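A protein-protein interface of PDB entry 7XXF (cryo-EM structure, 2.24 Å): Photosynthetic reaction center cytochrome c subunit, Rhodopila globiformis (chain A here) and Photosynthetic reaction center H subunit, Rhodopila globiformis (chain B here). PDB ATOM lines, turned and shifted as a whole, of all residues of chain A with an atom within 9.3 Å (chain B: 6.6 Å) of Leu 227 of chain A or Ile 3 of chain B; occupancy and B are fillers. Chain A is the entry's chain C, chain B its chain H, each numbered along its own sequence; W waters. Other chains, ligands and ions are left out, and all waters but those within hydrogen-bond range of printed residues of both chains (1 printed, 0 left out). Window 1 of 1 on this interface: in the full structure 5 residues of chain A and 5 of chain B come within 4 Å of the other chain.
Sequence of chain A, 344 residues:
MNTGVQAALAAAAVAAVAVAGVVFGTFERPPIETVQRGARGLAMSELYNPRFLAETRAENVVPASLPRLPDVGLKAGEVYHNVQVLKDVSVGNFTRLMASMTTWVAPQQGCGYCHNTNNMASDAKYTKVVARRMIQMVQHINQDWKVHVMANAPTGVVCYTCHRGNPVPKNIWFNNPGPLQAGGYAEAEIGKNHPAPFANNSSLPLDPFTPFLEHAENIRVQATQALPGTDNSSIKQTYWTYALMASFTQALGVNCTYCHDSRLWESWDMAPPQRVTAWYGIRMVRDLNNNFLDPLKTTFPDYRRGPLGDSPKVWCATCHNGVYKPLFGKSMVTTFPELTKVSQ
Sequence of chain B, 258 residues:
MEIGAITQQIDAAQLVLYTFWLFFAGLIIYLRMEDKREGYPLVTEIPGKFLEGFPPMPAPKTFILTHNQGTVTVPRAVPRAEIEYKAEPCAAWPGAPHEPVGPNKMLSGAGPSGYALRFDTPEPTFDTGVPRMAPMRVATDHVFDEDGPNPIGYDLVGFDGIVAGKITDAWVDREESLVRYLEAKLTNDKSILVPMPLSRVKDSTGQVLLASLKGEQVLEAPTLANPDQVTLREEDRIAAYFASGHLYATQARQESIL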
ATOM      1  N   GLN A 222      10.963  20.543 -37.265  1.00  0.00           N
ATOM      2  CA  GLN A 222       9.719  20.229 -36.579  1.00  0.00           C
ATOM      3  C   GLN A 222       9.505  18.724 -36.469  1.00  0.00           C
ATOM      4  O   GLN A 222       9.867  17.955 -37.361  1.00  0.00           O
ATOM      5  CB  GLN A 222       8.530  20.865 -37.298  1.00  0.00           C
ATOM      6  CG  GLN A 222       8.406  22.361 -37.092  1.00  0.00           C
ATOM      7  CD  GLN A 222       7.053  22.895 -37.509  1.00  0.00           C
ATOM      8  OE1 GLN A 222       6.376  22.312 -38.350  1.00  0.00           O
ATOM      9  NE2 GLN A 222       6.649  24.005 -36.913  1.00  0.00           N
ATOM     10  N   ALA A 223       8.910  18.311 -35.354  1.00  0.00           N
ATOM     11  CA  ALA A 223       8.536  16.917 -35.175  1.00  0.00           C
ATOM     12  C   ALA A 223       7.298  16.586 -36.000  1.00  0.00           C
ATOM     13  O   ALA A 223       6.409  17.420 -36.190  1.00  0.00           O
ATOM     14  CB  ALA A 223       8.276  16.614 -33.700  1.00  0.00           C
ATOM     15  N   THR A 224       7.239  15.349 -36.487  1.00  0.00           N
ATOM     16  CA  THR A 224       6.131  14.893 -37.315  1.00  0.00           C
ATOM     17  C   THR A 224       5.044  14.184 -36.518  1.00  0.00           C
ATOM     18  O   THR A 224       4.122  13.622 -37.116  1.00  0.00           O
ATOM     19  CB  THR A 224       6.640  13.973 -38.429  1.00  0.00           C
ATOM     20  OG1 THR A 224       7.411  12.907 -37.863  1.00  0.00           O
ATOM     21  CG2 THR A 224       7.500  14.751 -39.415  1.00  0.00           C
ATOM     22  N   GLN A 225       5.126  14.195 -35.192  1.00  0.00           N
ATOM     23  CA  GLN A 225       4.097  13.608 -34.349  1.00  0.00           C
ATOM     24  C   GLN A 225       3.880  14.498 -33.134  1.00  0.00           C
ATOM     25  O   GLN A 225       4.702  15.358 -32.814  1.00  0.00           O
ATOM     26  CB  GLN A 225       4.461  12.184 -33.916  1.00  0.00           C
ATOM     27  CG  GLN A 225       5.608  12.111 -32.938  1.00  0.00           C
ATOM     28  CD  GLN A 225       5.874  10.702 -32.455  1.00  0.00           C
ATOM     29  OE1 GLN A 225       5.792   9.747 -33.224  1.00  0.00           O
ATOM     30  NE2 GLN A 225       6.191  10.565 -31.175  1.00  0.00           N
ATOM     31  N   ALA A 226       2.748  14.281 -32.462  1.00  0.00           N
ATOM     32  CA  ALA A 226       2.372  15.138 -31.342  1.00  0.00           C
ATOM     33  C   ALA A 226       3.343  15.011 -30.173  1.00  0.00           C
ATOM     34  O   ALA A 226       3.728  16.019 -29.572  1.00  0.00           O
ATOM     35  CB  ALA A 226       0.949  14.811 -30.892  1.00  0.00           C
ATOM     36  N   LEU A 227       3.750  13.794 -29.836  1.00  0.00           N
ATOM     37  CA  LEU A 227       4.498  13.549 -28.614  1.00  0.00           C
ATOM     38  C   LEU A 227       5.985  13.387 -28.901  1.00  0.00           C
ATOM     39  O   LEU A 227       6.382  13.037 -30.014  1.00  0.00           O
ATOM     40  CB  LEU A 227       3.958  12.299 -27.910  1.00  0.00           C
ATOM     41  CG  LEU A 227       2.473  12.344 -27.539  1.00  0.00           C
ATOM     42  CD1 LEU A 227       2.098  11.179 -26.643  1.00  0.00           C
ATOM     43  CD2 LEU A 227       2.105  13.665 -26.885  1.00  0.00           C
ATOM     44  N   PRO A 228       6.842  13.645 -27.913  1.00  0.00           N
ATOM     45  CA  PRO A 228       8.288  13.566 -28.145  1.00  0.00           C
ATOM     46  C   PRO A 228       8.747  12.134 -28.370  1.00  0.00           C
ATOM     47  O   PRO A 228       8.026  11.165 -28.132  1.00  0.00           O
ATOM     48  CB  PRO A 228       8.892  14.141 -26.860  1.00  0.00           C
ATOM     49  CG  PRO A 228       7.786  14.889 -26.210  1.00  0.00           C
ATOM     50  CD  PRO A 228       6.540  14.160 -26.570  1.00  0.00           C
ATOM     51  N   GLY A 229       9.982  12.018 -28.848  1.00  0.00           N
ATOM     52  CA  GLY A 229      10.607  10.725 -29.030  1.00  0.00           C
ATOM     53  C   GLY A 229      11.241  10.526 -30.390  1.00  0.00           C
ATOM     54  O   GLY A 229      12.044   9.609 -30.573  1.00  0.00           O
ATOM     55  N   THR A 230      10.898  11.379 -31.354  1.00  0.00           N
ATOM     56  CA  THR A 230      11.360  11.213 -32.724  1.00  0.00           C
ATOM     57  C   THR A 230      12.170  12.391 -33.247  1.00  0.00           C
ATOM     58  O   THR A 230      12.668  12.324 -34.376  1.00  0.00           O
ATOM     59  CB  THR A 230      10.168  10.979 -33.664  1.00  0.00           C
ATOM     60  OG1 THR A 230       9.366  12.164 -33.723  1.00  0.00           O
ATOM     61  CG2 THR A 230       9.317   9.827 -33.167  1.00  0.00           C
ATOM     62  N   ASP A 231      12.323  13.459 -32.470  1.00  0.00           N
ATOM     63  CA  ASP A 231      12.912  14.694 -32.967  1.00  0.00           C
ATOM     64  C   ASP A 231      13.846  15.258 -31.911  1.00  0.00           C
ATOM     65  O   ASP A 231      13.418  15.531 -30.787  1.00  0.00           O
ATOM     66  CB  ASP A 231      11.818  15.704 -33.321  1.00  0.00           C
ATOM     67  CG  ASP A 231      12.355  16.943 -34.001  1.00  0.00           C
ATOM     68  OD1 ASP A 231      13.561  16.989 -34.314  1.00  0.00           O
ATOM     69  OD2 ASP A 231      11.558  17.874 -34.223  1.00  0.00           O
ATOM     70  N   MET B   1       7.950   5.403 -30.139  1.00  0.00           N
ATOM     71  CA  MET B   1       8.388   6.549 -29.349  1.00  0.00           C
ATOM     72  C   MET B   1       7.237   7.507 -29.072  1.00  0.00           C
ATOM     73  O   MET B   1       6.968   8.418 -29.854  1.00  0.00           O
ATOM     74  CB  MET B   1       9.525   7.285 -30.058  1.00  0.00           C
ATOM     75  CG  MET B   1      10.908   6.754 -29.725  1.00  0.00           C
ATOM     76  SD  MET B   1      11.308   6.952 -27.977  1.00  0.00           S
ATOM     77  CE  MET B   1      13.030   6.454 -27.956  1.00  0.00           C
ATOM     78  N   GLU B   2       6.556   7.293 -27.948  1.00  0.00           N
ATOM     79  CA  GLU B   2       5.452   8.141 -27.504  1.00  0.00           C
ATOM     80  C   GLU B   2       5.709   8.514 -26.047  1.00  0.00           C
ATOM     81  O   GLU B   2       5.226   7.857 -25.125  1.00  0.00           O
ATOM     82  CB  GLU B   2       4.118   7.424 -27.679  1.00  0.00           C
ATOM     83  CG  GLU B   2       3.795   7.065 -29.119  1.00  0.00           C
ATOM     84  CD  GLU B   2       3.284   8.249 -29.912  1.00  0.00           C
ATOM     85  OE1 GLU B   2       2.305   8.879 -29.467  1.00  0.00           O
ATOM     86  OE2 GLU B   2       3.862   8.551 -30.975  1.00  0.00           O
ATOM     87  N   ILE B   3       6.475   9.583 -25.847  1.00  0.00           N
ATOM     88  CA  ILE B   3       6.745  10.070 -24.502  1.00  0.00           C
ATOM     89  C   ILE B   3       5.605  10.974 -24.056  1.00  0.00           C
ATOM     90  O   ILE B   3       5.187  11.881 -24.787  1.00  0.00           O
ATOM     91  CB  ILE B   3       8.095  10.798 -24.454  1.00  0.00           C
ATOM     92  CG1 ILE B   3       9.234   9.797 -24.645  1.00  0.00           C
ATOM     93  CG2 ILE B   3       8.251  11.561 -23.149  1.00  0.00           C
ATOM     94  CD1 ILE B   3      10.595  10.429 -24.676  1.00  0.00           C
ATOM     95  N   GLY B   4       5.090  10.725 -22.859  1.00  0.00           N
ATOM     96  CA  GLY B   4       3.988  11.491 -22.322  1.00  0.00           C
ATOM     97  C   GLY B   4       2.624  10.869 -22.503  1.00  0.00           C
ATOM     98  O   GLY B   4       1.629  11.488 -22.116  1.00  0.00           O
ATOM     99  N   ALA B   5       2.541   9.669 -23.070  1.00  0.00           N
ATOM    100  CA  ALA B   5       1.264   9.012 -23.306  1.00  0.00           C
ATOM    101  C   ALA B   5       0.834   8.246 -22.063  1.00  0.00           C
ATOM    102  O   ALA B   5       1.613   7.467 -21.506  1.00  0.00           O
ATOM    103  CB  ALA B   5       1.355   8.065 -24.503  1.00  0.00           C
ATOM    104  N   ILE B   6      -0.399   8.481 -21.627  1.00  0.00           N
ATOM    105  CA  ILE B   6      -0.989   7.712 -20.535  1.00  0.00           C
ATOM    106  C   ILE B   6      -1.817   6.557 -21.074  1.00  0.00           C
ATOM    107  O   ILE B   6      -1.656   5.408 -20.656  1.00  0.00           O
ATOM    108  CB  ILE B   6      -1.832   8.635 -19.631  1.00  0.00           C
ATOM    109  CG1 ILE B   6      -1.031   9.877 -19.235  1.00  0.00           C
ATOM    110  CG2 ILE B   6      -2.295   7.890 -18.394  1.00  0.00           C
ATOM    111  CD1 ILE B   6       0.205   9.575 -18.434  1.00  0.00           C
ATOM    112  N   THR B   7      -2.717   6.855 -22.006  1.00  0.00           N
ATOM    113  CA  THR B   7      -3.406   5.847 -22.798  1.00  0.00           C
ATOM    114  C   THR B   7      -3.174   6.176 -24.265  1.00  0.00           C
ATOM    115  O   THR B   7      -2.350   7.038 -24.582  1.00  0.00           O
ATOM    116  CB  THR B   7      -4.903   5.803 -22.486  1.00  0.00           C
ATOM    117  OG1 THR B   7      -5.518   7.030 -22.896  1.00  0.00           O
ATOM    118  CG2 THR B   7      -5.137   5.601 -21.000  1.00  0.00           C
ATOM    119  N   ILE B  10      -5.176   9.728 -24.107  1.00  0.00           N
ATOM    120  CA  ILE B  10      -4.890  10.665 -23.026  1.00  0.00           C
ATOM    121  C   ILE B  10      -3.385  10.763 -22.833  1.00  0.00           C
ATOM    122  O   ILE B  10      -2.701   9.745 -22.678  1.00  0.00           O
ATOM    123  CB  ILE B  10      -5.591  10.236 -21.727  1.00  0.00           C
ATOM    124  CG1 ILE B  10      -7.101  10.421 -21.858  1.00  0.00           C
ATOM    125  CG2 ILE B  10      -5.065  11.029 -20.542  1.00  0.00           C
ATOM    126  CD1 ILE B  10      -7.876  10.037 -20.624  1.00  0.00           C
ATOM    127  N   ASP B  11      -2.866  11.986 -22.847  1.00  0.00           N
ATOM    128  CA  ASP B  11      -1.449  12.242 -22.645  1.00  0.00           C
ATOM    129  C   ASP B  11      -1.252  13.149 -21.435  1.00  0.00           C
ATOM    130  O   ASP B  11      -2.208  13.659 -20.847  1.00  0.00           O
ATOM    131  CB  ASP B  11      -0.808  12.849 -23.900  1.00  0.00           C
ATOM    132  CG  ASP B  11      -1.581  14.033 -24.441  1.00  0.00           C
ATOM    133  OD1 ASP B  11      -1.628  15.079 -23.764  1.00  0.00           O
ATOM    134  OD2 ASP B  11      -2.135  13.919 -25.551  1.00  0.00           O
ATOM    135  N   ALA B  12       0.016  13.336 -21.063  1.00  0.00           N
ATOM    136  CA  ALA B  12       0.335  14.038 -19.822  1.00  0.00           C
ATOM    137  C   ALA B  12      -0.116  15.493 -19.861  1.00  0.00           C
ATOM    138  O   ALA B  12      -0.658  16.004 -18.876  1.00  0.00           O
ATOM    139  CB  ALA B  12       1.834  13.951 -19.541  1.00  0.00           C
HETATM  140  O   HOH W   1       2.684  11.317 -30.996  1.00  0.00           O
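Printed residues of chain B within 4 Å of Gln 225 of chain A: Met 1 (2.6 Å) and Glu 2 (3.1 Å). Of chain B, only Glu 2, Ile 3 and Ala 5 come within 4 Å of Leu 227 of chain A. Printed residues of chain B within 4 Å of Pro 228 of chain A: Met 1 (3.4 Å) and Ile 3 (3.2 Å). Printed residues of chain B within 4 Å of Gly 229 of chain A: Met 1. Of the printed residues of chain A, Met 1 of chain B touches Gln 225, Pro 228 and Gly 229. Of chain A, only Gln 225 (3.1 Å) and Leu 227 (3.6 Å) come within 4 Å of Glu 2 of chain B. Printed residues of chain A within 4 Å of Ala 5 of chain B: Leu 227 (3.9 Å). The nearest residue of chain B that does not touch Leu 227 of chain A is Gly 4 of chain B (4.2 Å). The nearest residue of chain A that does not touch Ile 3 of chain B is Gly 229 of chain A (4.4 Å). The nearest printed residue of chain B that does not touch Gln 225 of chain A is Ile 3 of chain B (5.4 Å).
Of the 10 printed residues of chain B, 4 touch a printed residue of chain A.
NE2 of Gln 225 of chain A lies within hydrogen-bond range of O of Leu 227 of chain A (2.7 Å).
Among the printed residues, merely in contact across the chains: Leu 227 of chain A with Ile 3 of chain B, Leu 227 of chain A with Glu 2 of chain B and Leu 227 of chain A with Ala 5 of chain B.
O of Pro 228 of chain A is in hydrogen-bond range of N of Ile 3 of chain B, 3.2 Å away. The side-chain sulfur (SD) of Met 1 of chain B sits close to the backbone carbonyl oxygen (O) of Gly 229 of chain A, at 3.8 Å. O of Pro 228 of chain A lies close to O of Met 1 of chain B (3.4 Å). O of Met 1 of chain B lies within hydrogen-bond range of NE2 of Gln 225 of chain A (2.6 Å). NE2 of Gln 225 of chain A is in hydrogen-bond range of OE2 of Glu 2 of chain B.
Water W1 lies within hydrogen-bond range of OE1 of Glu 2 of chain B (2.9 Å), N of Leu 227 of chain A (2.9 Å) and N of Ala 226 of chain A (3.3 Å).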
